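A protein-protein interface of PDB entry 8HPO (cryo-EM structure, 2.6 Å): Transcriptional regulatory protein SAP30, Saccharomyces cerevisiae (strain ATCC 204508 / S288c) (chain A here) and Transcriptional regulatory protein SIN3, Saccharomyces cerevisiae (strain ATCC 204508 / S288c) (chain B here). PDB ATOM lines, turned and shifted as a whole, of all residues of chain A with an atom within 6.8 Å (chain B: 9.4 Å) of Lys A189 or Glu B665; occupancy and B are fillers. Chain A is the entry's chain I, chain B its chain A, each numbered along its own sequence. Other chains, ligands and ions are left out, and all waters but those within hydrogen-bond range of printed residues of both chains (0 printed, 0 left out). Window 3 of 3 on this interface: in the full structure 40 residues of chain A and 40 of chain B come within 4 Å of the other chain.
CD1 of Phe A184 touches CZ of Phe B669 (3.9 Å). Tyr B692 touches Phe A184. Phe A184 touches Phe B720 (CZ to CE2, 3.9 Å). CG2 of Ile A185 touches OE2 of Glu B665 (3.8 Å). NZ of Lys A187 touches CZ of Tyr B692 (3.5 Å). Val A188 touches Phe B723 (CG1 to O, 3.4 Å).
The backbone carbonyl oxygen (O) of Val B724 sits at hydrogen-bond distance from the side-chain amide nitrogen (NE2) of Gln A191. NE2 of Gln A191 is in hydrogen-bond range of OH of Tyr B692 (3.1 Å). OE2 of Glu B665 lies within salt-bridge range of NZ of Lys A189, 2.9 Å away.
Printed residues of chain B that touch a printed residue of chain A: Glu B665, Phe B669, Tyr B692, Phe B720, Phe B723 and Val B724. Hydrophobic or aromatic side chains of chain B within 4 Å of the printed part of chain A: Phe B669, Tyr B692 and Phe B720. Of the 10 printed residues of chain A, 6 touch a printed residue of chain B. Hydrophobic or aromatic side chains of chain A that line the printed part of chain B: Phe A184, Ile A185 and Val A188. Among the printed residues, 9 pairs touch across the chains. Among the printed residues, Asp or Glu carboxylates within 4 Å of a Lys or Arg side-chain nitrogen of the other chain: Lys A189 with Glu B665 (2.9 Å).
Printed residues of chain B within 4 Å of Phe A184: Phe B669 (3.9 Å), Tyr B692 (3.5 Å) and Phe B720 (3.9 Å). Of the printed residues of chain B, Lys A187 touches Tyr B692 (3.5 Å). Of chain B, only Phe B723 (3.4 Å) comes within 4 Å of Val A188. Of the printed residues of chain B, Lys A189 touches Glu B665. Glu B665 touches just these residues of chain A: Ile A185 (3.8 Å) and Lys A189 (2.9 Å). Val B666 touches none of the printed residues of chain A. Ala B672 touches none of the printed residues of chain A. Printed residues of chain A within 4 Å of Tyr B692: Phe A184, Lys A187 and Gln A191. Of the printed residues of chain A, Phe B720 touches Phe A184. Of the printed residues of chain A, Phe B723 touches Val A188. The nearest printed residue of chain A that does not touch Glu B665 is Tyr A186 (7.4 Å). The nearest printed residue of chain B that does not touch Phe A184 is Phe B723 (4.5 Å).
The side-chain amide oxygen (OE1) of Gln A191 sits close to the backbone carbonyl oxygen (O) of Val A188 (3.4 Å).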
ATOM      1  N   PHE A 184      17.598  17.159 -30.397  1.00  0.00           N
ATOM      2  CA  PHE A 184      18.900  17.790 -30.229  1.00  0.00           C
ATOM      3  C   PHE A 184      20.006  16.754 -30.090  1.00  0.00           C
ATOM      4  O   PHE A 184      21.066  16.879 -30.715  1.00  0.00           O
ATOM      5  CB  PHE A 184      18.878  18.715 -29.016  1.00  0.00           C
ATOM      6  CG  PHE A 184      20.139  19.495 -28.841  1.00  0.00           C
ATOM      7  CD1 PHE A 184      20.930  19.311 -27.725  1.00  0.00           C
ATOM      8  CD2 PHE A 184      20.543  20.406 -29.801  1.00  0.00           C
ATOM      9  CE1 PHE A 184      22.096  20.024 -27.565  1.00  0.00           C
ATOM     10  CE2 PHE A 184      21.709  21.120 -29.646  1.00  0.00           C
ATOM     11  CZ  PHE A 184      22.486  20.928 -28.528  1.00  0.00           C
ATOM     12  N   ILE A 185      19.789  15.736 -29.256  1.00  0.00           N
ATOM     13  CA  ILE A 185      20.811  14.715 -29.055  1.00  0.00           C
ATOM     14  C   ILE A 185      21.063  13.936 -30.339  1.00  0.00           C
ATOM     15  O   ILE A 185      22.217  13.676 -30.706  1.00  0.00           O
ATOM     16  CB  ILE A 185      20.415  13.787 -27.899  1.00  0.00           C
ATOM     17  CG1 ILE A 185      20.386  14.565 -26.588  1.00  0.00           C
ATOM     18  CG2 ILE A 185      21.363  12.615 -27.806  1.00  0.00           C
ATOM     19  CD1 ILE A 185      19.960  13.735 -25.427  1.00  0.00           C
ATOM     20  N   TYR A 186      20.001  13.553 -31.048  1.00  0.00           N
ATOM     21  CA  TYR A 186      20.209  12.833 -32.298  1.00  0.00           C
ATOM     22  C   TYR A 186      20.946  13.701 -33.307  1.00  0.00           C
ATOM     23  O   TYR A 186      21.706  13.192 -34.138  1.00  0.00           O
ATOM     24  CB  TYR A 186      18.878  12.356 -32.878  1.00  0.00           C
ATOM     25  CG  TYR A 186      19.044  11.563 -34.154  1.00  0.00           C
ATOM     26  CD1 TYR A 186      19.101  12.186 -35.385  1.00  0.00           C
ATOM     27  CD2 TYR A 186      19.151  10.195 -34.121  1.00  0.00           C
ATOM     28  CE1 TYR A 186      19.267  11.464 -36.541  1.00  0.00           C
ATOM     29  CE2 TYR A 186      19.314   9.468 -35.271  1.00  0.00           C
ATOM     30  CZ  TYR A 186      19.372  10.105 -36.477  1.00  0.00           C
ATOM     31  OH  TYR A 186      19.530   9.366 -37.619  1.00  0.00           O
ATOM     32  N   LYS A 187      20.735  15.014 -33.247  1.00  0.00           N
ATOM     33  CA  LYS A 187      21.393  15.914 -34.186  1.00  0.00           C
ATOM     34  C   LYS A 187      22.876  16.021 -33.877  1.00  0.00           C
ATOM     35  O   LYS A 187      23.721  15.832 -34.759  1.00  0.00           O
ATOM     36  CB  LYS A 187      20.724  17.285 -34.127  1.00  0.00           C
ATOM     37  CG  LYS A 187      21.351  18.333 -35.000  1.00  0.00           C
ATOM     38  CD  LYS A 187      20.926  18.181 -36.441  1.00  0.00           C
ATOM     39  CE  LYS A 187      21.841  18.976 -37.347  1.00  0.00           C
ATOM     40  NZ  LYS A 187      22.239  20.248 -36.703  1.00  0.00           N
ATOM     41  N   VAL A 188      23.204  16.292 -32.614  1.00  0.00           N
ATOM     42  CA  VAL A 188      24.597  16.455 -32.205  1.00  0.00           C
ATOM     43  C   VAL A 188      25.390  15.175 -32.442  1.00  0.00           C
ATOM     44  O   VAL A 188      26.537  15.217 -32.901  1.00  0.00           O
ATOM     45  CB  VAL A 188      24.664  16.903 -30.736  1.00  0.00           C
ATOM     46  CG1 VAL A 188      26.018  16.607 -30.148  1.00  0.00           C
ATOM     47  CG2 VAL A 188      24.348  18.376 -30.629  1.00  0.00           C
ATOM     48  N   LYS A 189      24.800  14.018 -32.146  1.00  0.00           N
ATOM     49  CA  LYS A 189      25.561  12.786 -32.311  1.00  0.00           C
ATOM     50  C   LYS A 189      25.691  12.340 -33.759  1.00  0.00           C
ATOM     51  O   LYS A 189      26.301  11.296 -34.002  1.00  0.00           O
ATOM     52  CB  LYS A 189      24.930  11.668 -31.488  1.00  0.00           C
ATOM     53  CG  LYS A 189      25.112  11.838 -30.000  1.00  0.00           C
ATOM     54  CD  LYS A 189      24.290  10.837 -29.219  1.00  0.00           C
ATOM     55  CE  LYS A 189      25.173  10.015 -28.295  1.00  0.00           C
ATOM     56  NZ  LYS A 189      25.640  10.810 -27.124  1.00  0.00           N
ATOM     57  N   ASN A 190      25.148  13.084 -34.722  1.00  0.00           N
ATOM     58  CA  ASN A 190      25.205  12.683 -36.124  1.00  0.00           C
ATOM     59  C   ASN A 190      25.731  13.798 -37.017  1.00  0.00           C
ATOM     60  O   ASN A 190      25.562  13.727 -38.237  1.00  0.00           O
ATOM     61  CB  ASN A 190      23.833  12.232 -36.626  1.00  0.00           C
ATOM     62  CG  ASN A 190      23.302  11.036 -35.882  1.00  0.00           C
ATOM     63  OD1 ASN A 190      23.322   9.917 -36.390  1.00  0.00           O
ATOM     64  ND2 ASN A 190      22.807  11.265 -34.675  1.00  0.00           N
ATOM     65  N   GLN A 191      26.356  14.825 -36.431  1.00  0.00           N
ATOM     66  CA  GLN A 191      26.816  15.980 -37.198  1.00  0.00           C
ATOM     67  C   GLN A 191      27.622  15.569 -38.421  1.00  0.00           C
ATOM     68  O   GLN A 191      27.476  16.161 -39.496  1.00  0.00           O
ATOM     69  CB  GLN A 191      27.657  16.892 -36.313  1.00  0.00           C
ATOM     70  CG  GLN A 191      26.869  17.777 -35.385  1.00  0.00           C
ATOM     71  CD  GLN A 191      27.686  18.204 -34.194  1.00  0.00           C
ATOM     72  OE1 GLN A 191      28.704  17.593 -33.881  1.00  0.00           O
ATOM     73  NE2 GLN A 191      27.252  19.259 -33.525  1.00  0.00           N
ATOM     74  N   LYS A 192      28.478  14.569 -38.282  1.00  0.00           N
ATOM     75  CA  LYS A 192      29.349  14.177 -39.375  1.00  0.00           C
ATOM     76  C   LYS A 192      28.637  13.353 -40.430  1.00  0.00           C
ATOM     77  O   LYS A 192      29.224  13.090 -41.483  1.00  0.00           O
ATOM     78  CB  LYS A 192      30.545  13.392 -38.839  1.00  0.00           C
ATOM     79  CG  LYS A 192      31.541  14.233 -38.067  1.00  0.00           C
ATOM     80  CD  LYS A 192      31.459  13.954 -36.578  1.00  0.00           C
ATOM     81  CE  LYS A 192      32.262  14.969 -35.797  1.00  0.00           C
ATOM     82  NZ  LYS A 192      32.269  16.284 -36.490  1.00  0.00           N
ATOM     83  N   LYS A 193      27.396  12.949 -40.181  1.00  0.00           N
ATOM     84  CA  LYS A 193      26.672  12.051 -41.067  1.00  0.00           C
ATOM     85  C   LYS A 193      25.956  12.845 -42.148  1.00  0.00           C
ATOM     86  O   LYS A 193      25.363  13.893 -41.869  1.00  0.00           O
ATOM     87  CB  LYS A 193      25.668  11.210 -40.281  1.00  0.00           C
ATOM     88  CG  LYS A 193      26.242   9.923 -39.742  1.00  0.00           C
ATOM     89  CD  LYS A 193      26.947   9.148 -40.835  1.00  0.00           C
ATOM     90  CE  LYS A 193      27.713   7.965 -40.268  1.00  0.00           C
ATOM     91  NZ  LYS A 193      28.717   7.449 -41.236  1.00  0.00           N
ATOM     92  N   ILE B 660      21.982   4.304 -26.765  1.00  0.00           N
ATOM     93  CA  ILE B 660      22.662   3.630 -25.668  1.00  0.00           C
ATOM     94  C   ILE B 660      23.490   4.623 -24.863  1.00  0.00           C
ATOM     95  O   ILE B 660      24.149   5.500 -25.424  1.00  0.00           O
ATOM     96  CB  ILE B 660      23.544   2.471 -26.187  1.00  0.00           C
ATOM     97  CG1 ILE B 660      24.705   3.009 -27.028  1.00  0.00           C
ATOM     98  CG2 ILE B 660      22.716   1.496 -27.011  1.00  0.00           C
ATOM     99  CD1 ILE B 660      26.043   2.376 -26.715  1.00  0.00           C
ATOM    100  N   SER B 661      23.420   4.496 -23.537  1.00  0.00           N
ATOM    101  CA  SER B 661      24.312   5.207 -22.623  1.00  0.00           C
ATOM    102  C   SER B 661      24.228   6.724 -22.812  1.00  0.00           C
ATOM    103  O   SER B 661      25.183   7.381 -23.225  1.00  0.00           O
ATOM    104  CB  SER B 661      25.755   4.714 -22.778  1.00  0.00           C
ATOM    105  OG  SER B 661      25.807   3.321 -23.019  1.00  0.00           O
ATOM    106  N   LEU B 662      23.054   7.272 -22.504  1.00  0.00           N
ATOM    107  CA  LEU B 662      22.825   8.711 -22.526  1.00  0.00           C
ATOM    108  C   LEU B 662      22.722   9.295 -21.122  1.00  0.00           C
ATOM    109  O   LEU B 662      21.859  10.137 -20.857  1.00  0.00           O
ATOM    110  CB  LEU B 662      21.573   9.041 -23.337  1.00  0.00           C
ATOM    111  CG  LEU B 662      21.387   8.255 -24.637  1.00  0.00           C
ATOM    112  CD1 LEU B 662      20.128   8.710 -25.343  1.00  0.00           C
ATOM    113  CD2 LEU B 662      22.598   8.404 -25.549  1.00  0.00           C
ATOM    114  N   ASN B 663      23.592   8.852 -20.213  1.00  0.00           N
ATOM    115  CA  ASN B 663      23.488   9.253 -18.813  1.00  0.00           C
ATOM    116  C   ASN B 663      23.956  10.687 -18.600  1.00  0.00           C
ATOM    117  O   ASN B 663      23.199  11.529 -18.100  1.00  0.00           O
ATOM    118  CB  ASN B 663      24.293   8.293 -17.940  1.00  0.00           C
ATOM    119  CG  ASN B 663      23.487   7.088 -17.499  1.00  0.00           C
ATOM    120  OD1 ASN B 663      23.584   6.010 -18.087  1.00  0.00           O
ATOM    121  ND2 ASN B 663      22.682   7.266 -16.458  1.00  0.00           N
ATOM    122  N   GLU B 664      25.204  10.987 -18.965  1.00  0.00           N
ATOM    123  CA  GLU B 664      25.772  12.286 -18.618  1.00  0.00           C
ATOM    124  C   GLU B 664      25.181  13.400 -19.469  1.00  0.00           C
ATOM    125  O   GLU B 664      25.201  14.566 -19.070  1.00  0.00           O
ATOM    126  CB  GLU B 664      27.297  12.250 -18.738  1.00  0.00           C
ATOM    127  CG  GLU B 664      27.850  12.334 -20.152  1.00  0.00           C
ATOM    128  CD  GLU B 664      27.822  10.999 -20.885  1.00  0.00           C
ATOM    129  OE1 GLU B 664      28.812  10.687 -21.579  1.00  0.00           O
ATOM    130  OE2 GLU B 664      26.817  10.265 -20.780  1.00  0.00           O
ATOM    131  N   GLU B 665      24.629  13.064 -20.632  1.00  0.00           N
ATOM    132  CA  GLU B 665      23.955  14.077 -21.438  1.00  0.00           C
ATOM    133  C   GLU B 665      22.702  14.601 -20.743  1.00  0.00           C
ATOM    134  O   GLU B 665      22.564  15.812 -20.504  1.00  0.00           O
ATOM    135  CB  GLU B 665      23.623  13.491 -22.805  1.00  0.00           C
ATOM    136  CG  GLU B 665      24.861  13.079 -23.571  1.00  0.00           C
ATOM    137  CD  GLU B 665      24.717  11.749 -24.274  1.00  0.00           C
ATOM    138  OE1 GLU B 665      25.589  10.879 -24.080  1.00  0.00           O
ATOM    139  OE2 GLU B 665      23.746  11.575 -25.034  1.00  0.00           O
ATOM    140  N   VAL B 666      21.778  13.704 -20.399  1.00  0.00           N
ATOM    141  CA  VAL B 666      20.602  14.126 -19.652  1.00  0.00           C
ATOM    142  C   VAL B 666      20.999  14.656 -18.280  1.00  0.00           C
ATOM    143  O   VAL B 666      20.284  15.476 -17.699  1.00  0.00           O
ATOM    144  CB  VAL B 666      19.592  12.973 -19.552  1.00  0.00           C
ATOM    145  CG1 VAL B 666      19.448  12.285 -20.898  1.00  0.00           C
ATOM    146  CG2 VAL B 666      20.029  11.987 -18.507  1.00  0.00           C
ATOM    147  N   THR B 667      22.152  14.232 -17.751  1.00  0.00           N
ATOM    148  CA  THR B 667      22.637  14.812 -16.503  1.00  0.00           C
ATOM    149  C   THR B 667      23.038  16.271 -16.680  1.00  0.00           C
ATOM    150  O   THR B 667      22.757  17.103 -15.806  1.00  0.00           O
ATOM    151  CB  THR B 667      23.817  14.002 -15.972  1.00  0.00           C
ATOM    152  OG1 THR B 667      23.575  12.610 -16.198  1.00  0.00           O
ATOM    153  CG2 THR B 667      23.996  14.242 -14.488  1.00  0.00           C
ATOM    154  N   PHE B 668      23.704  16.595 -17.794  1.00  0.00           N
ATOM    155  CA  PHE B 668      23.974  17.988 -18.126  1.00  0.00           C
ATOM    156  C   PHE B 668      22.677  18.761 -18.232  1.00  0.00           C
ATOM    157  O   PHE B 668      22.592  19.916 -17.809  1.00  0.00           O
ATOM    158  CB  PHE B 668      24.747  18.099 -19.442  1.00  0.00           C
ATOM    159  CG  PHE B 668      24.543  19.417 -20.153  1.00  0.00           C
ATOM    160  CD1 PHE B 668      23.951  19.463 -21.402  1.00  0.00           C
ATOM    161  CD2 PHE B 668      24.949  20.608 -19.573  1.00  0.00           C
ATOM    162  CE1 PHE B 668      23.761  20.664 -22.052  1.00  0.00           C
ATOM    163  CE2 PHE B 668      24.754  21.813 -20.220  1.00  0.00           C
ATOM    164  CZ  PHE B 668      24.160  21.837 -21.460  1.00  0.00           C
ATOM    165  N   PHE B 669      21.657  18.144 -18.821  1.00  0.00           N
ATOM    166  CA  PHE B 669      20.387  18.851 -18.928  1.00  0.00           C
ATOM    167  C   PHE B 669      19.744  19.060 -17.561  1.00  0.00           C
ATOM    168  O   PHE B 669      19.106  20.095 -17.334  1.00  0.00           O
ATOM    169  CB  PHE B 669      19.456  18.116 -19.882  1.00  0.00           C
ATOM    170  CG  PHE B 669      19.598  18.562 -21.302  1.00  0.00           C
ATOM    171  CD1 PHE B 669      19.069  19.771 -21.710  1.00  0.00           C
ATOM    172  CD2 PHE B 669      20.282  17.792 -22.224  1.00  0.00           C
ATOM    173  CE1 PHE B 669      19.208  20.198 -23.010  1.00  0.00           C
ATOM    174  CE2 PHE B 669      20.422  18.215 -23.530  1.00  0.00           C
ATOM    175  CZ  PHE B 669      19.884  19.418 -23.922  1.00  0.00           C
ATOM    176  N   GLU B 670      19.923  18.111 -16.639  1.00  0.00           N
ATOM    177  CA  GLU B 670      19.494  18.312 -15.257  1.00  0.00           C
ATOM    178  C   GLU B 670      20.179  19.534 -14.657  1.00  0.00           C
ATOM    179  O   GLU B 670      19.528  20.440 -14.117  1.00  0.00           O
ATOM    180  CB  GLU B 670      19.818  17.076 -14.413  1.00  0.00           C
ATOM    181  CG  GLU B 670      19.236  15.744 -14.867  1.00  0.00           C
ATOM    182  CD  GLU B 670      17.879  15.848 -15.527  1.00  0.00           C
ATOM    183  OE1 GLU B 670      17.650  15.120 -16.515  1.00  0.00           O
ATOM    184  OE2 GLU B 670      17.020  16.600 -15.023  1.00  0.00           O
ATOM    185  N   LYS B 671      21.512  19.555 -14.738  1.00  0.00           N
ATOM    186  CA  LYS B 671      22.281  20.682 -14.220  1.00  0.00           C
ATOM    187  C   LYS B 671      21.864  21.997 -14.866  1.00  0.00           C
ATOM    188  O   LYS B 671      21.790  23.022 -14.183  1.00  0.00           O
ATOM    189  CB  LYS B 671      23.777  20.442 -14.428  1.00  0.00           C
ATOM    190  CG  LYS B 671      24.273  19.074 -13.979  1.00  0.00           C
ATOM    191  CD  LYS B 671      23.911  18.794 -12.531  1.00  0.00           C
ATOM    192  CE  LYS B 671      24.775  19.597 -11.574  1.00  0.00           C
ATOM    193  NZ  LYS B 671      26.070  18.925 -11.287  1.00  0.00           N
ATOM    194  N   ALA B 672      21.575  21.988 -16.168  1.00  0.00           N
ATOM    195  CA  ALA B 672      21.244  23.225 -16.868  1.00  0.00           C
ATOM    196  C   ALA B 672      19.868  23.738 -16.466  1.00  0.00           C
ATOM    197  O   ALA B 672      19.690  24.940 -16.235  1.00  0.00           O
ATOM    198  CB  ALA B 672      21.318  23.007 -18.376  1.00  0.00           C
ATOM    199  N   LYS B 673      18.885  22.840 -16.372  1.00  0.00           N
ATOM    200  CA  LYS B 673      17.577  23.238 -15.867  1.00  0.00           C
ATOM    201  C   LYS B 673      17.685  23.777 -14.448  1.00  0.00           C
ATOM    202  O   LYS B 673      16.977  24.724 -14.082  1.00  0.00           O
ATOM    203  CB  LYS B 673      16.608  22.059 -15.921  1.00  0.00           C
ATOM    204  CG  LYS B 673      15.145  22.469 -15.959  1.00  0.00           C
ATOM    205  CD  LYS B 673      14.220  21.262 -15.978  1.00  0.00           C
ATOM    206  CE  LYS B 673      14.141  20.642 -17.362  1.00  0.00           C
ATOM    207  NZ  LYS B 673      13.195  19.494 -17.406  1.00  0.00           N
ATOM    208  N   TYR B 692      18.840  25.299 -33.413  1.00  0.00           N
ATOM    209  CA  TYR B 692      20.000  24.590 -33.949  1.00  0.00           C
ATOM    210  C   TYR B 692      19.593  23.258 -34.566  1.00  0.00           C
ATOM    211  O   TYR B 692      19.931  22.969 -35.718  1.00  0.00           O
ATOM    212  CB  TYR B 692      21.058  24.358 -32.880  1.00  0.00           C
ATOM    213  CG  TYR B 692      22.196  23.518 -33.418  1.00  0.00           C
ATOM    214  CD1 TYR B 692      22.507  22.284 -32.865  1.00  0.00           C
ATOM    215  CD2 TYR B 692      22.936  23.947 -34.506  1.00  0.00           C
ATOM    216  CE1 TYR B 692      23.533  21.514 -33.374  1.00  0.00           C
ATOM    217  CE2 TYR B 692      23.960  23.189 -35.017  1.00  0.00           C
ATOM    218  CZ  TYR B 692      24.257  21.974 -34.449  1.00  0.00           C
ATOM    219  OH  TYR B 692      25.280  21.219 -34.965  1.00  0.00           O
ATOM    220  N   LEU B 716      29.943  23.619 -17.207  1.00  0.00           N
ATOM    221  CA  LEU B 716      28.803  23.388 -18.086  1.00  0.00           C
ATOM    222  C   LEU B 716      29.167  23.725 -19.520  1.00  0.00           C
ATOM    223  O   LEU B 716      28.909  22.948 -20.445  1.00  0.00           O
ATOM    224  CB  LEU B 716      27.611  24.232 -17.636  1.00  0.00           C
ATOM    225  CG  LEU B 716      26.758  23.737 -16.468  1.00  0.00           C
ATOM    226  CD1 LEU B 716      25.524  24.609 -16.307  1.00  0.00           C
ATOM    227  CD2 LEU B 716      26.367  22.287 -16.677  1.00  0.00           C
ATOM    228  N   TRP B 719      31.826  21.251 -21.111  1.00  0.00           N
ATOM    229  CA  TRP B 719      31.178  19.978 -21.407  1.00  0.00           C
ATOM    230  C   TRP B 719      30.275  20.114 -22.621  1.00  0.00           C
ATOM    231  O   TRP B 719      30.248  19.237 -23.488  1.00  0.00           O
ATOM    232  CB  TRP B 719      30.371  19.474 -20.211  1.00  0.00           C
ATOM    233  CG  TRP B 719      29.864  18.082 -20.455  1.00  0.00           C
ATOM    234  CD1 TRP B 719      30.494  16.915 -20.138  1.00  0.00           C
ATOM    235  CD2 TRP B 719      28.659  17.714 -21.135  1.00  0.00           C
ATOM    236  NE1 TRP B 719      29.742  15.844 -20.552  1.00  0.00           N
ATOM    237  CE2 TRP B 719      28.613  16.309 -21.170  1.00  0.00           C
ATOM    238  CE3 TRP B 719      27.608  18.435 -21.706  1.00  0.00           C
ATOM    239  CZ2 TRP B 719      27.559  15.615 -21.749  1.00  0.00           C
ATOM    240  CZ3 TRP B 719      26.570  17.744 -22.286  1.00  0.00           C
ATOM    241  CH2 TRP B 719      26.547  16.350 -22.296  1.00  0.00           C
ATOM    242  N   PHE B 720      29.513  21.208 -22.687  1.00  0.00           N
ATOM    243  CA  PHE B 720      28.672  21.469 -23.849  1.00  0.00           C
ATOM    244  C   PHE B 720      29.499  21.538 -25.125  1.00  0.00           C
ATOM    245  O   PHE B 720      29.171  20.886 -26.122  1.00  0.00           O
ATOM    246  CB  PHE B 720      27.900  22.771 -23.636  1.00  0.00           C
ATOM    247  CG  PHE B 720      26.939  23.097 -24.736  1.00  0.00           C
ATOM    248  CD1 PHE B 720      27.152  24.189 -25.556  1.00  0.00           C
ATOM    249  CD2 PHE B 720      25.812  22.322 -24.943  1.00  0.00           C
ATOM    250  CE1 PHE B 720      26.266  24.496 -26.567  1.00  0.00           C
ATOM    251  CE2 PHE B 720      24.925  22.624 -25.951  1.00  0.00           C
ATOM    252  CZ  PHE B 720      25.153  23.711 -26.765  1.00  0.00           C
ATOM    253  N   ASN B 722      32.521  20.412 -25.836  1.00  0.00           N
ATOM    254  CA  ASN B 722      33.012  19.091 -26.208  1.00  0.00           C
ATOM    255  C   ASN B 722      31.892  18.224 -26.762  1.00  0.00           C
ATOM    256  O   ASN B 722      32.104  17.471 -27.718  1.00  0.00           O
ATOM    257  CB  ASN B 722      33.645  18.395 -25.007  1.00  0.00           C
ATOM    258  CG  ASN B 722      34.795  19.172 -24.422  1.00  0.00           C
ATOM    259  OD1 ASN B 722      35.071  20.299 -24.829  1.00  0.00           O
ATOM    260  ND2 ASN B 722      35.469  18.575 -23.450  1.00  0.00           N
ATOM    261  N   PHE B 723      30.706  18.315 -26.158  1.00  0.00           N
ATOM    262  CA  PHE B 723      29.538  17.575 -26.617  1.00  0.00           C
ATOM    263  C   PHE B 723      29.206  17.921 -28.063  1.00  0.00           C
ATOM    264  O   PHE B 723      29.126  17.040 -28.923  1.00  0.00           O
ATOM    265  CB  PHE B 723      28.359  17.877 -25.687  1.00  0.00           C
ATOM    266  CG  PHE B 723      27.165  16.998 -25.896  1.00  0.00           C
ATOM    267  CD1 PHE B 723      25.892  17.534 -25.861  1.00  0.00           C
ATOM    268  CD2 PHE B 723      27.309  15.641 -26.119  1.00  0.00           C
ATOM    269  CE1 PHE B 723      24.786  16.743 -26.052  1.00  0.00           C
ATOM    270  CE2 PHE B 723      26.203  14.842 -26.312  1.00  0.00           C
ATOM    271  CZ  PHE B 723      24.940  15.397 -26.278  1.00  0.00           C
ATOM    272  N   VAL B 724      29.034  19.213 -28.353  1.00  0.00           N
ATOM    273  CA  VAL B 724      28.627  19.632 -29.690  1.00  0.00           C
ATOM    274  C   VAL B 724      29.737  19.459 -30.715  1.00  0.00           C
ATOM    275  O   VAL B 724      29.457  19.419 -31.917  1.00  0.00           O
ATOM    276  CB  VAL B 724      28.134  21.091 -29.685  1.00  0.00           C
ATOM    277  CG1 VAL B 724      27.160  21.322 -28.550  1.00  0.00           C
ATOM    278  CG2 VAL B 724      29.297  22.037 -29.577  1.00  0.00           C
ATOM    279  N   GLY B 725      30.991  19.363 -30.286  1.00  0.00           N
ATOM    280  CA  GLY B 725      32.084  19.183 -31.221  1.00  0.00           C
ATOM    281  C   GLY B 725      32.724  20.495 -31.610  1.00  0.00           C
ATOM    282  O   GLY B 725      33.063  20.716 -32.775  1.00  0.00           O
